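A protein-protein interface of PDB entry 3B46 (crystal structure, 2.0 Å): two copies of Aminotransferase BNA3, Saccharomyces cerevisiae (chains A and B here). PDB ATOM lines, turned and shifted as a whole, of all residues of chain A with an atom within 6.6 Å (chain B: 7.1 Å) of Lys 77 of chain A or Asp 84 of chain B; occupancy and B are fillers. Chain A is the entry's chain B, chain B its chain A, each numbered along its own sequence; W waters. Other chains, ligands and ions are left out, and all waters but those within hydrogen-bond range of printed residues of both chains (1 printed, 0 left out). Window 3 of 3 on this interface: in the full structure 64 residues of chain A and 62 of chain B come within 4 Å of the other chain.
The backbone carbonyl oxygen (O) of Leu 83 of chain B is in hydrogen-bond range of the side-chain amide nitrogen (ND2) of Asn 89 of chain B (3.1 Å). The backbone carbonyl oxygen (O) of Ile 85 of chain B is in hydrogen-bond range of the side-chain amide nitrogen (ND2) of Asn 89 of chain B, 3.4 Å away. O of Pro 86 of chain B sits close to ND2 of Asn 89 of chain B (3.4 Å). OE1 of Gln 73 of chain A lies within hydrogen-bond range of NZ of Lys 77 of chain A, at 2.7 Å.
Printed residues of chain B that touch a printed residue of chain A: Gln 80, Leu 83, Asp 84, Pro 86 and Asn 89. Hydrophobic or aromatic side chains of chain B within 4 Å of the printed part of chain A: Leu 83 and Pro 86. Hydrophobic or aromatic side chains of chain A that line the printed part of chain B: Ile 76 and Ala 79. Among the printed residues, Asp or Glu carboxylates within 4 Å of a Lys or Arg side-chain nitrogen of the other chain: Lys 77 of chain A with Asp 84 of chain B.
Gln 80 of chain A touches its own counterpart, Gln 80 of chain B. Positions printed for both chains: 78, 79, 80, 81 and 82.
The side-chain amide nitrogen (NE2) of Gln 80 of chain B is in hydrogen-bond range of the backbone carbonyl oxygen (O) of Gln 80 of chain A, at 2.7 Å. The side-chain amino group (NZ) of Lys 77 of chain A lies within salt-bridge range of the side-chain carboxylate (OD2) of Asp 84 of chain B, 3.96 Å away. The side-chain carboxylate (OD1) of Asp 84 of chain B sits at hydrogen-bond distance from the side-chain amide nitrogen (NE2) of Gln 80 of chain A (3.2 Å).
Of the printed residues of chain B, Ile 76 of chain A touches Leu 83, Asp 84 and Asn 89. Of chain B, only Asp 84 (3.96 Å) comes within 4 Å of Lys 77 of chain A. Of the printed residues of chain A, Gln 80 of chain B touches Gln 80 (2.7 Å). Of the printed residues of chain A, Leu 83 of chain B touches Ile 76, Ala 79 and Gln 80. Printed residues of chain A within 4 Å of Asp 84 of chain B: Ile 76 (3.99 Å), Lys 77 (3.96 Å) and Gln 80 (3.2 Å). The nearest residue of chain B that does not touch Lys 77 of chain A is Leu 83 of chain B (6.7 Å). The nearest printed residue of chain B that does not touch Gln 80 of chain A is Lys 81 of chain B (4.9 Å).
Water W1 lies within hydrogen-bond range of OG of Ser 70 of chain A, O of Leu 83 of chain B, ND2 of Asn 89 of chain B and O of Asp 84 of chain B.
Among the printed residues, pairs that only touch across the chains: Ser 70 of chain A with Pro 86 of chain B, Ile 76 of chain A with Leu 83 of chain B, Ile 76 of chain A with Asp 84 of chain B, Ile 76 of chain A with Asn 89 of chain B, Ala 79 of chain A with Leu 83 of chain B and Gln 80 of chain A with Leu 83 of chain B.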
ATOM      1  N   SER A  70      15.824   4.313   9.842  1.00  0.00           N
ATOM      2  CA  SER A  70      16.864   4.194  10.857  1.00  0.00           C
ATOM      3  C   SER A  70      16.505   4.800  12.197  1.00  0.00           C
ATOM      4  O   SER A  70      15.648   5.667  12.275  1.00  0.00           O
ATOM      5  CB  SER A  70      18.162   4.866  10.376  1.00  0.00           C
ATOM      6  OG  SER A  70      19.044   5.130  11.475  1.00  0.00           O
ATOM      7  N   PRO A  72      16.952   7.212  15.424  1.00  0.00           N
ATOM      8  CA  PRO A  72      17.477   8.582  15.402  1.00  0.00           C
ATOM      9  C   PRO A  72      19.003   8.602  15.339  1.00  0.00           C
ATOM     10  O   PRO A  72      19.686   7.748  15.912  1.00  0.00           O
ATOM     11  CB  PRO A  72      16.914   9.190  16.690  1.00  0.00           C
ATOM     12  CG  PRO A  72      16.762   7.996  17.591  1.00  0.00           C
ATOM     13  CD  PRO A  72      16.186   6.960  16.654  1.00  0.00           C
ATOM     14  N   GLN A  73      19.540   9.576  14.627  1.00  0.00           N
ATOM     15  CA  GLN A  73      20.974   9.637  14.481  1.00  0.00           C
ATOM     16  C   GLN A  73      21.678   9.684  15.843  1.00  0.00           C
ATOM     17  O   GLN A  73      22.800   9.168  15.969  1.00  0.00           O
ATOM     18  CB  GLN A  73      21.365  10.835  13.605  1.00  0.00           C
ATOM     19  CG  GLN A  73      22.764  10.722  13.015  1.00  0.00           C
ATOM     20  CD  GLN A  73      22.962   9.452  12.179  1.00  0.00           C
ATOM     21  OE1 GLN A  73      24.096   9.051  11.911  1.00  0.00           O
ATOM     22  NE2 GLN A  73      21.861   8.824  11.762  1.00  0.00           N
ATOM     23  N   PHE A  74      21.030  10.258  16.861  1.00  0.00           N
ATOM     24  CA  PHE A  74      21.675  10.323  18.179  1.00  0.00           C
ATOM     25  C   PHE A  74      21.876   8.938  18.786  1.00  0.00           C
ATOM     26  O   PHE A  74      22.860   8.708  19.475  1.00  0.00           O
ATOM     27  CB  PHE A  74      20.916  11.242  19.151  1.00  0.00           C
ATOM     28  CG  PHE A  74      19.657  10.648  19.741  1.00  0.00           C
ATOM     29  CD1 PHE A  74      19.719   9.776  20.822  1.00  0.00           C
ATOM     30  CD2 PHE A  74      18.407  10.987  19.227  1.00  0.00           C
ATOM     31  CE1 PHE A  74      18.549   9.249  21.383  1.00  0.00           C
ATOM     32  CE2 PHE A  74      17.238  10.464  19.782  1.00  0.00           C
ATOM     33  CZ  PHE A  74      17.313   9.594  20.859  1.00  0.00           C
ATOM     34  N   ALA A  75      20.953   8.015  18.525  1.00  0.00           N
ATOM     35  CA  ALA A  75      21.089   6.641  19.032  1.00  0.00           C
ATOM     36  C   ALA A  75      22.184   5.923  18.242  1.00  0.00           C
ATOM     37  O   ALA A  75      22.990   5.187  18.804  1.00  0.00           O
ATOM     38  CB  ALA A  75      19.773   5.881  18.879  1.00  0.00           C
ATOM     39  N   ILE A  76      22.206   6.128  16.932  1.00  0.00           N
ATOM     40  CA  ILE A  76      23.213   5.484  16.099  1.00  0.00           C
ATOM     41  C   ILE A  76      24.605   5.858  16.596  1.00  0.00           C
ATOM     42  O   ILE A  76      25.485   5.009  16.752  1.00  0.00           O
ATOM     43  CB  ILE A  76      23.088   5.926  14.632  1.00  0.00           C
ATOM     44  CG1 ILE A  76      21.737   5.476  14.061  1.00  0.00           C
ATOM     45  CG2 ILE A  76      24.240   5.336  13.819  1.00  0.00           C
ATOM     46  CD1 ILE A  76      21.556   3.962  14.016  1.00  0.00           C
ATOM     47  N   LYS A  77      24.801   7.146  16.833  1.00  0.00           N
ATOM     48  CA  LYS A  77      26.082   7.637  17.321  1.00  0.00           C
ATOM     49  C   LYS A  77      26.447   7.091  18.697  1.00  0.00           C
ATOM     50  O   LYS A  77      27.611   6.827  18.962  1.00  0.00           O
ATOM     51  CB  LYS A  77      26.073   9.176  17.352  1.00  0.00           C
ATOM     52  CG  LYS A  77      26.708   9.832  16.127  1.00  0.00           C
ATOM     53  CD  LYS A  77      26.227   9.201  14.813  1.00  0.00           C
ATOM     54  CE  LYS A  77      27.084   9.653  13.629  1.00  0.00           C
ATOM     55  NZ  LYS A  77      26.734   8.902  12.377  1.00  0.00           N
ATOM     56  N   GLU A  78      25.470   6.932  19.586  1.00  0.00           N
ATOM     57  CA  GLU A  78      25.779   6.412  20.919  1.00  0.00           C
ATOM     58  C   GLU A  78      26.248   4.968  20.778  1.00  0.00           C
ATOM     59  O   GLU A  78      27.120   4.508  21.522  1.00  0.00           O
ATOM     60  CB  GLU A  78      24.555   6.468  21.836  1.00  0.00           C
ATOM     61  CG  GLU A  78      24.084   7.883  22.185  1.00  0.00           C
ATOM     62  CD  GLU A  78      25.061   8.636  23.094  1.00  0.00           C
ATOM     63  OE1 GLU A  78      26.183   8.144  23.319  1.00  0.00           O
ATOM     64  OE2 GLU A  78      24.701   9.732  23.575  1.00  0.00           O
ATOM     65  N   ALA A  79      25.666   4.263  19.804  1.00  0.00           N
ATOM     66  CA  ALA A  79      26.009   2.868  19.543  1.00  0.00           C
ATOM     67  C   ALA A  79      27.403   2.720  18.954  1.00  0.00           C
ATOM     68  O   ALA A  79      28.156   1.833  19.351  1.00  0.00           O
ATOM     69  CB  ALA A  79      24.968   2.229  18.604  1.00  0.00           C
ATOM     70  N   GLN A  80      27.783   3.585  18.025  1.00  0.00           N
ATOM     71  CA  GLN A  80      29.125   3.431  17.446  1.00  0.00           C
ATOM     72  C   GLN A  80      30.207   3.791  18.476  1.00  0.00           C
ATOM     73  O   GLN A  80      31.255   3.165  18.552  1.00  0.00           O
ATOM     74  CB  GLN A  80      29.245   4.297  16.195  1.00  0.00           C
ATOM     75  CG  GLN A  80      28.231   3.936  15.131  1.00  0.00           C
ATOM     76  CD  GLN A  80      28.211   4.945  14.018  1.00  0.00           C
ATOM     77  OE1 GLN A  80      28.124   6.148  14.267  1.00  0.00           O
ATOM     78  NE2 GLN A  80      28.281   4.468  12.782  1.00  0.00           N
ATOM     79  N   LYS A  81      29.914   4.799  19.286  1.00  0.00           N
ATOM     80  CA  LYS A  81      30.818   5.255  20.331  1.00  0.00           C
ATOM     81  C   LYS A  81      30.990   4.162  21.391  1.00  0.00           C
ATOM     82  O   LYS A  81      32.105   3.868  21.836  1.00  0.00           O
ATOM     83  CB  LYS A  81      30.242   6.542  20.948  1.00  0.00           C
ATOM     84  CG  LYS A  81      31.113   7.189  21.989  1.00  0.00           C
ATOM     85  CD  LYS A  81      30.406   8.389  22.626  1.00  0.00           C
ATOM     86  CE  LYS A  81      31.141   8.816  23.882  1.00  0.00           C
ATOM     87  NZ  LYS A  81      31.500   7.629  24.728  1.00  0.00           N
ATOM     88  N   ALA A  82      29.879   3.544  21.781  1.00  0.00           N
ATOM     89  CA  ALA A  82      29.912   2.493  22.780  1.00  0.00           C
ATOM     90  C   ALA A  82      30.857   1.358  22.406  1.00  0.00           C
ATOM     91  O   ALA A  82      31.552   0.813  23.263  1.00  0.00           O
ATOM     92  CB  ALA A  82      28.507   1.955  23.017  1.00  0.00           C
ATOM     93  N   GLU B  78      33.566  -3.146  11.720  1.00  0.00           N
ATOM     94  CA  GLU B  78      32.422  -3.721  11.010  1.00  0.00           C
ATOM     95  C   GLU B  78      31.109  -3.431  11.755  1.00  0.00           C
ATOM     96  O   GLU B  78      30.073  -3.182  11.135  1.00  0.00           O
ATOM     97  CB  GLU B  78      32.599  -5.229  10.869  1.00  0.00           C
ATOM     98  CG  GLU B  78      33.784  -5.651   9.995  1.00  0.00           C
ATOM     99  CD  GLU B  78      33.549  -5.381   8.512  1.00  0.00           C
ATOM    100  OE1 GLU B  78      32.610  -4.613   8.177  1.00  0.00           O
ATOM    101  OE2 GLU B  78      34.314  -5.940   7.686  1.00  0.00           O
ATOM    102  N   ALA B  79      31.150  -3.464  13.087  1.00  0.00           N
ATOM    103  CA  ALA B  79      29.950  -3.194  13.874  1.00  0.00           C
ATOM    104  C   ALA B  79      29.535  -1.716  13.749  1.00  0.00           C
ATOM    105  O   ALA B  79      28.342  -1.396  13.630  1.00  0.00           O
ATOM    106  CB  ALA B  79      30.189  -3.577  15.355  1.00  0.00           C
ATOM    107  N   GLN B  80      30.510  -0.808  13.768  1.00  0.00           N
ATOM    108  CA  GLN B  80      30.192   0.608  13.618  1.00  0.00           C
ATOM    109  C   GLN B  80      29.609   0.896  12.211  1.00  0.00           C
ATOM    110  O   GLN B  80      28.684   1.688  12.076  1.00  0.00           O
ATOM    111  CB  GLN B  80      31.445   1.452  13.903  1.00  0.00           C
ATOM    112  CG  GLN B  80      31.926   1.284  15.361  1.00  0.00           C
ATOM    113  CD  GLN B  80      33.218   2.011  15.670  1.00  0.00           C
ATOM    114  OE1 GLN B  80      34.156   2.021  14.864  1.00  0.00           O
ATOM    115  NE2 GLN B  80      33.285   2.606  16.854  1.00  0.00           N
ATOM    116  N   LYS B  81      30.146   0.244  11.180  1.00  0.00           N
ATOM    117  CA  LYS B  81      29.642   0.412   9.815  1.00  0.00           C
ATOM    118  C   LYS B  81      28.218  -0.093   9.720  1.00  0.00           C
ATOM    119  O   LYS B  81      27.338   0.579   9.184  1.00  0.00           O
ATOM    120  CB  LYS B  81      30.503  -0.374   8.809  1.00  0.00           C
ATOM    121  CG  LYS B  81      31.833   0.275   8.533  1.00  0.00           C
ATOM    122  CD  LYS B  81      32.814  -0.656   7.863  1.00  0.00           C
ATOM    123  CE  LYS B  81      32.757  -0.605   6.350  1.00  0.00           C
ATOM    124  NZ  LYS B  81      33.809  -1.530   5.822  1.00  0.00           N
ATOM    125  N   ALA B  82      28.006  -1.292  10.249  1.00  0.00           N
ATOM    126  CA  ALA B  82      26.701  -1.928  10.224  1.00  0.00           C
ATOM    127  C   ALA B  82      25.607  -1.019  10.779  1.00  0.00           C
ATOM    128  O   ALA B  82      24.488  -0.982  10.252  1.00  0.00           O
ATOM    129  CB  ALA B  82      26.754  -3.249  10.999  1.00  0.00           C
ATOM    130  N   LEU B  83      25.929  -0.270  11.828  1.00  0.00           N
ATOM    131  CA  LEU B  83      24.942   0.625  12.437  1.00  0.00           C
ATOM    132  C   LEU B  83      24.539   1.756  11.516  1.00  0.00           C
ATOM    133  O   LEU B  83      23.520   2.381  11.729  1.00  0.00           O
ATOM    134  CB  LEU B  83      25.485   1.212  13.750  1.00  0.00           C
ATOM    135  CG  LEU B  83      25.621   0.170  14.847  1.00  0.00           C
ATOM    136  CD1 LEU B  83      26.681   0.601  15.852  1.00  0.00           C
ATOM    137  CD2 LEU B  83      24.273  -0.048  15.494  1.00  0.00           C
ATOM    138  N   ASP B  84      25.346   2.029  10.497  1.00  0.00           N
ATOM    139  CA  ASP B  84      25.031   3.112   9.568  1.00  0.00           C
ATOM    140  C   ASP B  84      24.042   2.673   8.499  1.00  0.00           C
ATOM    141  O   ASP B  84      23.593   3.490   7.699  1.00  0.00           O
ATOM    142  CB  ASP B  84      26.303   3.650   8.893  1.00  0.00           C
ATOM    143  CG  ASP B  84      26.955   4.775   9.679  1.00  0.00           C
ATOM    144  OD1 ASP B  84      28.205   4.911   9.602  1.00  0.00           O
ATOM    145  OD2 ASP B  84      26.218   5.533  10.358  1.00  0.00           O
ATOM    146  N   ILE B  85      23.706   1.387   8.485  1.00  0.00           N
ATOM    147  CA  ILE B  85      22.759   0.858   7.503  1.00  0.00           C
ATOM    148  C   ILE B  85      21.384   0.779   8.167  1.00  0.00           C
ATOM    149  O   ILE B  85      21.110  -0.114   8.950  1.00  0.00           O
ATOM    150  CB  ILE B  85      23.190  -0.536   7.014  1.00  0.00           C
ATOM    151  CG1 ILE B  85      24.644  -0.495   6.539  1.00  0.00           C
ATOM    152  CG2 ILE B  85      22.279  -0.991   5.883  1.00  0.00           C
ATOM    153  CD1 ILE B  85      25.188  -1.862   6.117  1.00  0.00           C
ATOM    154  N   PRO B  86      20.496   1.722   7.840  1.00  0.00           N
ATOM    155  CA  PRO B  86      19.136   1.815   8.387  1.00  0.00           C
ATOM    156  C   PRO B  86      18.443   0.513   8.825  1.00  0.00           C
ATOM    157  O   PRO B  86      18.190   0.312  10.012  1.00  0.00           O
ATOM    158  CB  PRO B  86      18.378   2.536   7.277  1.00  0.00           C
ATOM    159  CG  PRO B  86      19.427   3.471   6.742  1.00  0.00           C
ATOM    160  CD  PRO B  86      20.627   2.560   6.630  1.00  0.00           C
ATOM    161  N   MET B  87      18.150  -0.366   7.866  1.00  0.00           N
ATOM    162  CA  MET B  87      17.436  -1.611   8.152  1.00  0.00           C
ATOM    163  C   MET B  87      18.224  -2.625   8.943  1.00  0.00           C
ATOM    164  O   MET B  87      17.662  -3.568   9.485  1.00  0.00           O
ATOM    165  CB  MET B  87      16.922  -2.252   6.847  1.00  0.00           C
ATOM    166  CG  MET B  87      15.820  -1.446   6.141  1.00  0.00           C
ATOM    167  SD  MET B  87      14.371  -1.104   7.183  1.00  0.00           S
ATOM    168  CE  MET B  87      13.689  -2.720   7.386  1.00  0.00           C
ATOM    169  N   VAL B  88      19.533  -2.452   8.983  1.00  0.00           N
ATOM    170  CA  VAL B  88      20.340  -3.358   9.755  1.00  0.00           C
ATOM    171  C   VAL B  88      20.030  -3.099  11.240  1.00  0.00           C
ATOM    172  O   VAL B  88      20.404  -3.873  12.091  1.00  0.00           O
ATOM    173  CB  VAL B  88      21.842  -3.171   9.429  1.00  0.00           C
ATOM    174  CG1 VAL B  88      22.716  -3.849  10.489  1.00  0.00           C
ATOM    175  CG2 VAL B  88      22.129  -3.812   8.059  1.00  0.00           C
ATOM    176  N   ASN B  89      19.321  -2.016  11.530  1.00  0.00           N
ATOM    177  CA  ASN B  89      18.956  -1.714  12.907  1.00  0.00           C
ATOM    178  C   ASN B  89      17.579  -2.275  13.232  1.00  0.00           C
ATOM    179  O   ASN B  89      17.087  -2.103  14.349  1.00  0.00           O
ATOM    180  CB  ASN B  89      18.967  -0.207  13.141  1.00  0.00           C
ATOM    181  CG  ASN B  89      20.368   0.353  13.182  1.00  0.00           C
ATOM    182  OD1 ASN B  89      21.122   0.101  14.123  1.00  0.00           O
ATOM    183  ND2 ASN B  89      20.738   1.097  12.143  1.00  0.00           N
HETATM  184  O   HOH W   1      21.187   3.757  10.117  1.00  0.00           O
